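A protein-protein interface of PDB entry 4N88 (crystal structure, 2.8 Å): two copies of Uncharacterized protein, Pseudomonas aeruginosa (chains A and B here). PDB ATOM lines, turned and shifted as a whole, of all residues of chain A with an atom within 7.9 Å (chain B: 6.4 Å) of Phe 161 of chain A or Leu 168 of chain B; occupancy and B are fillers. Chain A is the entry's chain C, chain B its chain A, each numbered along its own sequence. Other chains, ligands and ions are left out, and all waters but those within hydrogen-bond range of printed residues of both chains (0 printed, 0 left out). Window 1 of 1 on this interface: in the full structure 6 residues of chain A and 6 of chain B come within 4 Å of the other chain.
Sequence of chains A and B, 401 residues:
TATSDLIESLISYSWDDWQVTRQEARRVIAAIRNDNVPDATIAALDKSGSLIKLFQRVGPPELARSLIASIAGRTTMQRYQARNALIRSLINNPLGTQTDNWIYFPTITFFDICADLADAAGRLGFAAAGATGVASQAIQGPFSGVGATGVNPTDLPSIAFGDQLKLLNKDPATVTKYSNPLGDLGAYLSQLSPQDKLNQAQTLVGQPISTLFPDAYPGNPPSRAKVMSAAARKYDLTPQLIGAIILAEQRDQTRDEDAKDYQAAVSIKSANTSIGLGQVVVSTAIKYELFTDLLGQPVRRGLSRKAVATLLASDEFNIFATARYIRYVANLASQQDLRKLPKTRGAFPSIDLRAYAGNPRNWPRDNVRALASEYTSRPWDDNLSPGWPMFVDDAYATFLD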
ATOM      1  N   SER A 158      -3.234 -16.402 -11.950  1.00  0.00           N
ATOM      2  CA  SER A 158      -2.321 -15.337 -11.588  1.00  0.00           C
ATOM      3  C   SER A 158      -2.719 -14.797 -10.232  1.00  0.00           C
ATOM      4  O   SER A 158      -3.904 -14.725  -9.895  1.00  0.00           O
ATOM      5  CB  SER A 158      -2.375 -14.208 -12.617  1.00  0.00           C
ATOM      6  OG  SER A 158      -1.899 -14.635 -13.878  1.00  0.00           O
ATOM      7  N   ILE A 159      -1.729 -14.413  -9.447  1.00  0.00           N
ATOM      8  CA  ILE A 159      -2.024 -13.841  -8.149  1.00  0.00           C
ATOM      9  C   ILE A 159      -2.742 -12.501  -8.356  1.00  0.00           C
ATOM     10  O   ILE A 159      -2.318 -11.675  -9.171  1.00  0.00           O
ATOM     11  CB  ILE A 159      -0.738 -13.720  -7.289  1.00  0.00           C
ATOM     12  CG1 ILE A 159      -0.186 -15.132  -6.991  1.00  0.00           C
ATOM     13  CG2 ILE A 159      -1.023 -12.954  -6.010  1.00  0.00           C
ATOM     14  CD1 ILE A 159       1.216 -15.198  -6.369  1.00  0.00           C
ATOM     15  N   ALA A 160      -3.847 -12.308  -7.638  1.00  0.00           N
ATOM     16  CA  ALA A 160      -4.635 -11.072  -7.731  1.00  0.00           C
ATOM     17  C   ALA A 160      -3.778  -9.809  -7.547  1.00  0.00           C
ATOM     18  O   ALA A 160      -2.725  -9.839  -6.885  1.00  0.00           O
ATOM     19  CB  ALA A 160      -5.787 -11.093  -6.717  1.00  0.00           C
ATOM     20  N   PHE A 161      -4.241  -8.700  -8.121  1.00  0.00           N
ATOM     21  CA  PHE A 161      -3.482  -7.453  -8.084  1.00  0.00           C
ATOM     22  C   PHE A 161      -3.289  -6.912  -6.673  1.00  0.00           C
ATOM     23  O   PHE A 161      -2.221  -6.385  -6.351  1.00  0.00           O
ATOM     24  CB  PHE A 161      -4.115  -6.414  -9.008  1.00  0.00           C
ATOM     25  CG  PHE A 161      -3.928  -6.734 -10.462  1.00  0.00           C
ATOM     26  CD1 PHE A 161      -2.718  -7.275 -10.912  1.00  0.00           C
ATOM     27  CD2 PHE A 161      -4.953  -6.537 -11.379  1.00  0.00           C
ATOM     28  CE1 PHE A 161      -2.520  -7.592 -12.258  1.00  0.00           C
ATOM     29  CE2 PHE A 161      -4.766  -6.854 -12.729  1.00  0.00           C
ATOM     30  CZ  PHE A 161      -3.543  -7.381 -13.166  1.00  0.00           C
ATOM     31  N   GLY A 162      -4.314  -7.058  -5.833  1.00  0.00           N
ATOM     32  CA  GLY A 162      -4.225  -6.605  -4.458  1.00  0.00           C
ATOM     33  C   GLY A 162      -3.045  -7.260  -3.781  1.00  0.00           C
ATOM     34  O   GLY A 162      -2.208  -6.598  -3.150  1.00  0.00           O
ATOM     35  N   ASP A 163      -2.976  -8.577  -3.951  1.00  0.00           N
ATOM     36  CA  ASP A 163      -1.950  -9.399  -3.328  1.00  0.00           C
ATOM     37  C   ASP A 163      -0.554  -9.164  -3.901  1.00  0.00           C
ATOM     38  O   ASP A 163       0.415  -9.121  -3.151  1.00  0.00           O
ATOM     39  CB  ASP A 163      -2.338 -10.882  -3.413  1.00  0.00           C
ATOM     40  CG  ASP A 163      -3.349 -11.302  -2.331  1.00  0.00           C
ATOM     41  OD1 ASP A 163      -3.105 -10.985  -1.141  1.00  0.00           O
ATOM     42  OD2 ASP A 163      -4.370 -11.959  -2.674  1.00  0.00           O
ATOM     43  N   GLN A 164      -0.439  -9.015  -5.218  1.00  0.00           N
ATOM     44  CA  GLN A 164       0.870  -8.749  -5.827  1.00  0.00           C
ATOM     45  C   GLN A 164       1.450  -7.468  -5.281  1.00  0.00           C
ATOM     46  O   GLN A 164       2.661  -7.239  -5.334  1.00  0.00           O
ATOM     47  CB  GLN A 164       0.752  -8.548  -7.326  1.00  0.00           C
ATOM     48  CG  GLN A 164       0.221  -9.700  -8.094  1.00  0.00           C
ATOM     49  CD  GLN A 164       0.394  -9.482  -9.570  1.00  0.00           C
ATOM     50  OE1 GLN A 164      -0.495  -9.787 -10.366  1.00  0.00           O
ATOM     51  NE2 GLN A 164       1.548  -8.936  -9.951  1.00  0.00           N
ATOM     52  N   LEU A 165       0.551  -6.612  -4.809  1.00  0.00           N
ATOM     53  CA  LEU A 165       0.911  -5.299  -4.316  1.00  0.00           C
ATOM     54  C   LEU A 165       1.436  -5.458  -2.908  1.00  0.00           C
ATOM     55  O   LEU A 165       2.566  -5.050  -2.613  1.00  0.00           O
ATOM     56  CB  LEU A 165      -0.313  -4.381  -4.330  1.00  0.00           C
ATOM     57  CG  LEU A 165      -0.117  -2.895  -4.014  1.00  0.00           C
ATOM     58  CD1 LEU A 165       0.930  -2.293  -4.935  1.00  0.00           C
ATOM     59  CD2 LEU A 165      -1.452  -2.179  -4.141  1.00  0.00           C
ATOM     60  N   LYS A 166       0.619  -6.068  -2.046  1.00  0.00           N
ATOM     61  CA  LYS A 166       1.030  -6.329  -0.674  1.00  0.00           C
ATOM     62  C   LYS A 166       2.314  -7.159  -0.683  1.00  0.00           C
ATOM     63  O   LYS A 166       3.148  -7.050   0.218  1.00  0.00           O
ATOM     64  CB  LYS A 166      -0.076  -7.044   0.090  1.00  0.00           C
ATOM     65  CG  LYS A 166      -1.470  -6.547  -0.218  1.00  0.00           C
ATOM     66  CD  LYS A 166      -2.397  -6.738   0.972  1.00  0.00           C
ATOM     67  CE  LYS A 166      -3.869  -6.596   0.579  1.00  0.00           C
ATOM     68  NZ  LYS A 166      -4.342  -7.676  -0.363  1.00  0.00           N
ATOM     69  N   LEU A 167       2.476  -7.973  -1.724  1.00  0.00           N
ATOM     70  CA  LEU A 167       3.666  -8.798  -1.879  1.00  0.00           C
ATOM     71  C   LEU A 167       4.896  -8.013  -2.317  1.00  0.00           C
ATOM     72  O   LEU A 167       6.020  -8.498  -2.209  1.00  0.00           O
ATOM     73  CB  LEU A 167       3.397  -9.942  -2.851  1.00  0.00           C
ATOM     74  CG  LEU A 167       3.009 -11.275  -2.203  1.00  0.00           C
ATOM     75  CD1 LEU A 167       2.790 -12.329  -3.262  1.00  0.00           C
ATOM     76  CD2 LEU A 167       4.079 -11.715  -1.218  1.00  0.00           C
ATOM     77  N   LEU A 168       4.686  -6.798  -2.811  1.00  0.00           N
ATOM     78  CA  LEU A 168       5.797  -5.936  -3.220  1.00  0.00           C
ATOM     79  C   LEU A 168       6.216  -5.062  -2.038  1.00  0.00           C
ATOM     80  O   LEU A 168       7.399  -4.738  -1.862  1.00  0.00           O
ATOM     81  CB  LEU A 168       5.395  -5.067  -4.417  1.00  0.00           C
ATOM     82  CG  LEU A 168       6.446  -4.852  -5.510  1.00  0.00           C
ATOM     83  CD1 LEU A 168       6.761  -6.163  -6.248  1.00  0.00           C
ATOM     84  CD2 LEU A 168       5.964  -3.777  -6.480  1.00  0.00           C
ATOM     85  N   ASP B 163       3.385   1.387  -9.425  1.00  0.00           N
ATOM     86  CA  ASP B 163       2.344   2.374  -9.668  1.00  0.00           C
ATOM     87  C   ASP B 163       1.173   1.809 -10.471  1.00  0.00           C
ATOM     88  O   ASP B 163       0.015   2.055 -10.136  1.00  0.00           O
ATOM     89  CB  ASP B 163       2.948   3.604 -10.350  1.00  0.00           C
ATOM     90  CG  ASP B 163       3.420   4.656  -9.348  1.00  0.00           C
ATOM     91  OD1 ASP B 163       2.781   4.759  -8.276  1.00  0.00           O
ATOM     92  OD2 ASP B 163       4.413   5.379  -9.628  1.00  0.00           O
ATOM     93  N   GLN B 164       1.472   1.037 -11.514  1.00  0.00           N
ATOM     94  CA  GLN B 164       0.424   0.407 -12.311  1.00  0.00           C
ATOM     95  C   GLN B 164      -0.554  -0.341 -11.433  1.00  0.00           C
ATOM     96  O   GLN B 164      -1.758  -0.374 -11.697  1.00  0.00           O
ATOM     97  CB  GLN B 164       1.023  -0.585 -13.285  1.00  0.00           C
ATOM     98  CG  GLN B 164       2.029  -0.016 -14.214  1.00  0.00           C
ATOM     99  CD  GLN B 164       1.834  -0.557 -15.607  1.00  0.00           C
ATOM    100  OE1 GLN B 164       2.769  -0.604 -16.411  1.00  0.00           O
ATOM    101  NE2 GLN B 164       0.604  -0.974 -15.905  1.00  0.00           N
ATOM    102  N   LEU B 165      -0.009  -0.964 -10.395  1.00  0.00           N
ATOM    103  CA  LEU B 165      -0.762  -1.837  -9.513  1.00  0.00           C
ATOM    104  C   LEU B 165      -1.652  -1.032  -8.603  1.00  0.00           C
ATOM    105  O   LEU B 165      -2.830  -1.349  -8.435  1.00  0.00           O
ATOM    106  CB  LEU B 165       0.211  -2.644  -8.663  1.00  0.00           C
ATOM    107  CG  LEU B 165       0.199  -4.167  -8.700  1.00  0.00           C
ATOM    108  CD1 LEU B 165      -0.045  -4.697 -10.099  1.00  0.00           C
ATOM    109  CD2 LEU B 165       1.542  -4.613  -8.169  1.00  0.00           C
ATOM    110  N   LYS B 166      -1.071  -0.001  -7.994  1.00  0.00           N
ATOM    111  CA  LYS B 166      -1.839   0.937  -7.191  1.00  0.00           C
ATOM    112  C   LYS B 166      -3.003   1.528  -7.993  1.00  0.00           C
ATOM    113  O   LYS B 166      -4.107   1.628  -7.472  1.00  0.00           O
ATOM    114  CB  LYS B 166      -0.952   2.061  -6.676  1.00  0.00           C
ATOM    115  CG  LYS B 166       0.070   1.680  -5.627  1.00  0.00           C
ATOM    116  CD  LYS B 166       1.084   2.816  -5.477  1.00  0.00           C
ATOM    117  CE  LYS B 166       1.738   2.842  -4.115  1.00  0.00           C
ATOM    118  NZ  LYS B 166       2.597   1.637  -3.879  1.00  0.00           N
ATOM    119  N   LEU B 167      -2.764   1.912  -9.254  1.00  0.00           N
ATOM    120  CA  LEU B 167      -3.839   2.462 -10.107  1.00  0.00           C
ATOM    121  C   LEU B 167      -4.950   1.449 -10.307  1.00  0.00           C
ATOM    122  O   LEU B 167      -6.128   1.785 -10.224  1.00  0.00           O
ATOM    123  CB  LEU B 167      -3.329   2.978 -11.467  1.00  0.00           C
ATOM    124  CG  LEU B 167      -2.455   4.252 -11.459  1.00  0.00           C
ATOM    125  CD1 LEU B 167      -1.801   4.545 -12.815  1.00  0.00           C
ATOM    126  CD2 LEU B 167      -3.208   5.480 -10.943  1.00  0.00           C
ATOM    127  N   LEU B 168      -4.562   0.203 -10.554  1.00  0.00           N
ATOM    128  CA  LEU B 168      -5.517  -0.898 -10.697  1.00  0.00           C
ATOM    129  C   LEU B 168      -6.277  -1.154  -9.389  1.00  0.00           C
ATOM    130  O   LEU B 168      -7.405  -1.665  -9.398  1.00  0.00           O
ATOM    131  CB  LEU B 168      -4.794  -2.162 -11.151  1.00  0.00           C
ATOM    132  CG  LEU B 168      -5.269  -2.900 -12.406  1.00  0.00           C
ATOM    133  CD1 LEU B 168      -6.354  -2.155 -13.210  1.00  0.00           C
ATOM    134  CD2 LEU B 168      -4.053  -3.202 -13.269  1.00  0.00           C
ATOM    135  N   ASN B 169      -5.659  -0.780  -8.271  1.00  0.00           N
ATOM    136  CA  ASN B 169      -6.290  -0.941  -6.965  1.00  0.00           C
ATOM    137  C   ASN B 169      -7.049   0.313  -6.541  1.00  0.00           C
ATOM    138  O   ASN B 169      -7.545   0.394  -5.415  1.00  0.00           O
ATOM    139  CB  ASN B 169      -5.247  -1.330  -5.909  1.00  0.00           C
ATOM    140  CG  ASN B 169      -5.808  -2.265  -4.843  1.00  0.00           C
ATOM    141  OD1 ASN B 169      -6.259  -3.381  -5.149  1.00  0.00           O
ATOM    142  ND2 ASN B 169      -5.771  -1.819  -3.583  1.00  0.00           N
ATOM    143  N   LYS B 170      -7.128   1.282  -7.453  1.00  0.00           N
ATOM    144  CA  LYS B 170      -7.819   2.549  -7.210  1.00  0.00           C
ATOM    145  C   LYS B 170      -7.376   3.276  -5.922  1.00  0.00           C
ATOM    146  O   LYS B 170      -8.195   3.872  -5.210  1.00  0.00           O
ATOM    147  CB  LYS B 170      -9.336   2.360  -7.294  1.00  0.00           C
ATOM    148  CG  LYS B 170      -9.807   2.073  -8.723  1.00  0.00           C
ATOM    149  CD  LYS B 170     -11.239   1.538  -8.784  1.00  0.00           C
ATOM    150  CE  LYS B 170     -11.663   1.228 -10.233  1.00  0.00           C
ATOM    151  NZ  LYS B 170     -13.007   0.569 -10.355  1.00  0.00           N
ATOM    152  N   ASP B 171      -6.064   3.221  -5.662  1.00  0.00           N
ATOM    153  CA  ASP B 171      -5.395   3.948  -4.582  1.00  0.00           C
ATOM    154  C   ASP B 171      -5.510   5.464  -4.763  1.00  0.00           C
ATOM    155  O   ASP B 171      -4.934   6.016  -5.696  1.00  0.00           O
ATOM    156  CB  ASP B 171      -3.908   3.549  -4.561  1.00  0.00           C
ATOM    157  CG  ASP B 171      -3.101   4.290  -3.486  1.00  0.00           C
ATOM    158  OD1 ASP B 171      -3.707   4.798  -2.515  1.00  0.00           O
ATOM    159  OD2 ASP B 171      -1.854   4.359  -3.605  1.00  0.00           O
ATOM    160  N   LYS B 269      -7.346  -3.492 -20.792  1.00  0.00           N
ATOM    161  CA  LYS B 269      -8.613  -2.856 -20.412  1.00  0.00           C
ATOM    162  C   LYS B 269      -9.334  -2.176 -21.569  1.00  0.00           C
ATOM    163  O   LYS B 269     -10.559  -2.019 -21.527  1.00  0.00           O
ATOM    164  CB  LYS B 269      -8.372  -1.809 -19.319  1.00  0.00           C
ATOM    165  CG  LYS B 269      -7.669  -2.351 -18.082  1.00  0.00           C
ATOM    166  CD  LYS B 269      -7.152  -1.224 -17.182  1.00  0.00           C
ATOM    167  CE  LYS B 269      -6.197  -0.284 -17.937  1.00  0.00           C
ATOM    168  NZ  LYS B 269      -5.033   0.202 -17.115  1.00  0.00           N
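Phe 161 of chain A touches Leu 165 of chain B (CD1 to CD1, 3.8 Å).
CD2 of Leu 168 of chain B touches CE2 of Phe 161 of chain A, at 3.8 Å.
Gly 162 of chain A touches Asn 169 of chain B.
Leu 165 of chain A touches Leu 165 of chain B.
Phe 161 of chain A touches two residues of chain B.
Leu 168 of chain B touches just one residue of chain A: Phe 161 (3.8 Å).
Of the printed residues of chain B, Leu 165 of chain A touches Leu 165.
Of the printed residues of chain A, Leu 165 of chain B touches Phe 161 and Leu 165.
Printed residues of chain B within 4 Å of Gly 162 of chain A: Asn 169 (3.9 Å).
Of the printed residues of chain A, Asn 169 of chain B touches Gly 162 (3.9 Å).
Leu 168 of chain A touches none of the printed residues of chain B.
The nearest residue of chain B that does not touch Phe 161 of chain A is Asn 169 of chain B (4.9 Å).
Of the 10 printed residues of chain B, 3 touch a printed residue of chain A.
Along chain B the printed residues that touch a printed residue of chain A span positions 165 to 169.
Of the 11 printed residues of chain A, 3 touch a printed residue of chain B.
Hydrophobic or aromatic side chains of chain A within 4 Å of the printed part of chain B: Phe 161 and Leu 165.
Among the printed residues, 4 pairs touch across the chains.
Leu 165 of chain A touches its own counterpart, Leu 165 of chain B.
Of the 4 pairs that touch across the chains among the printed residues, 1 has its exchanged pair printed and touching as well.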
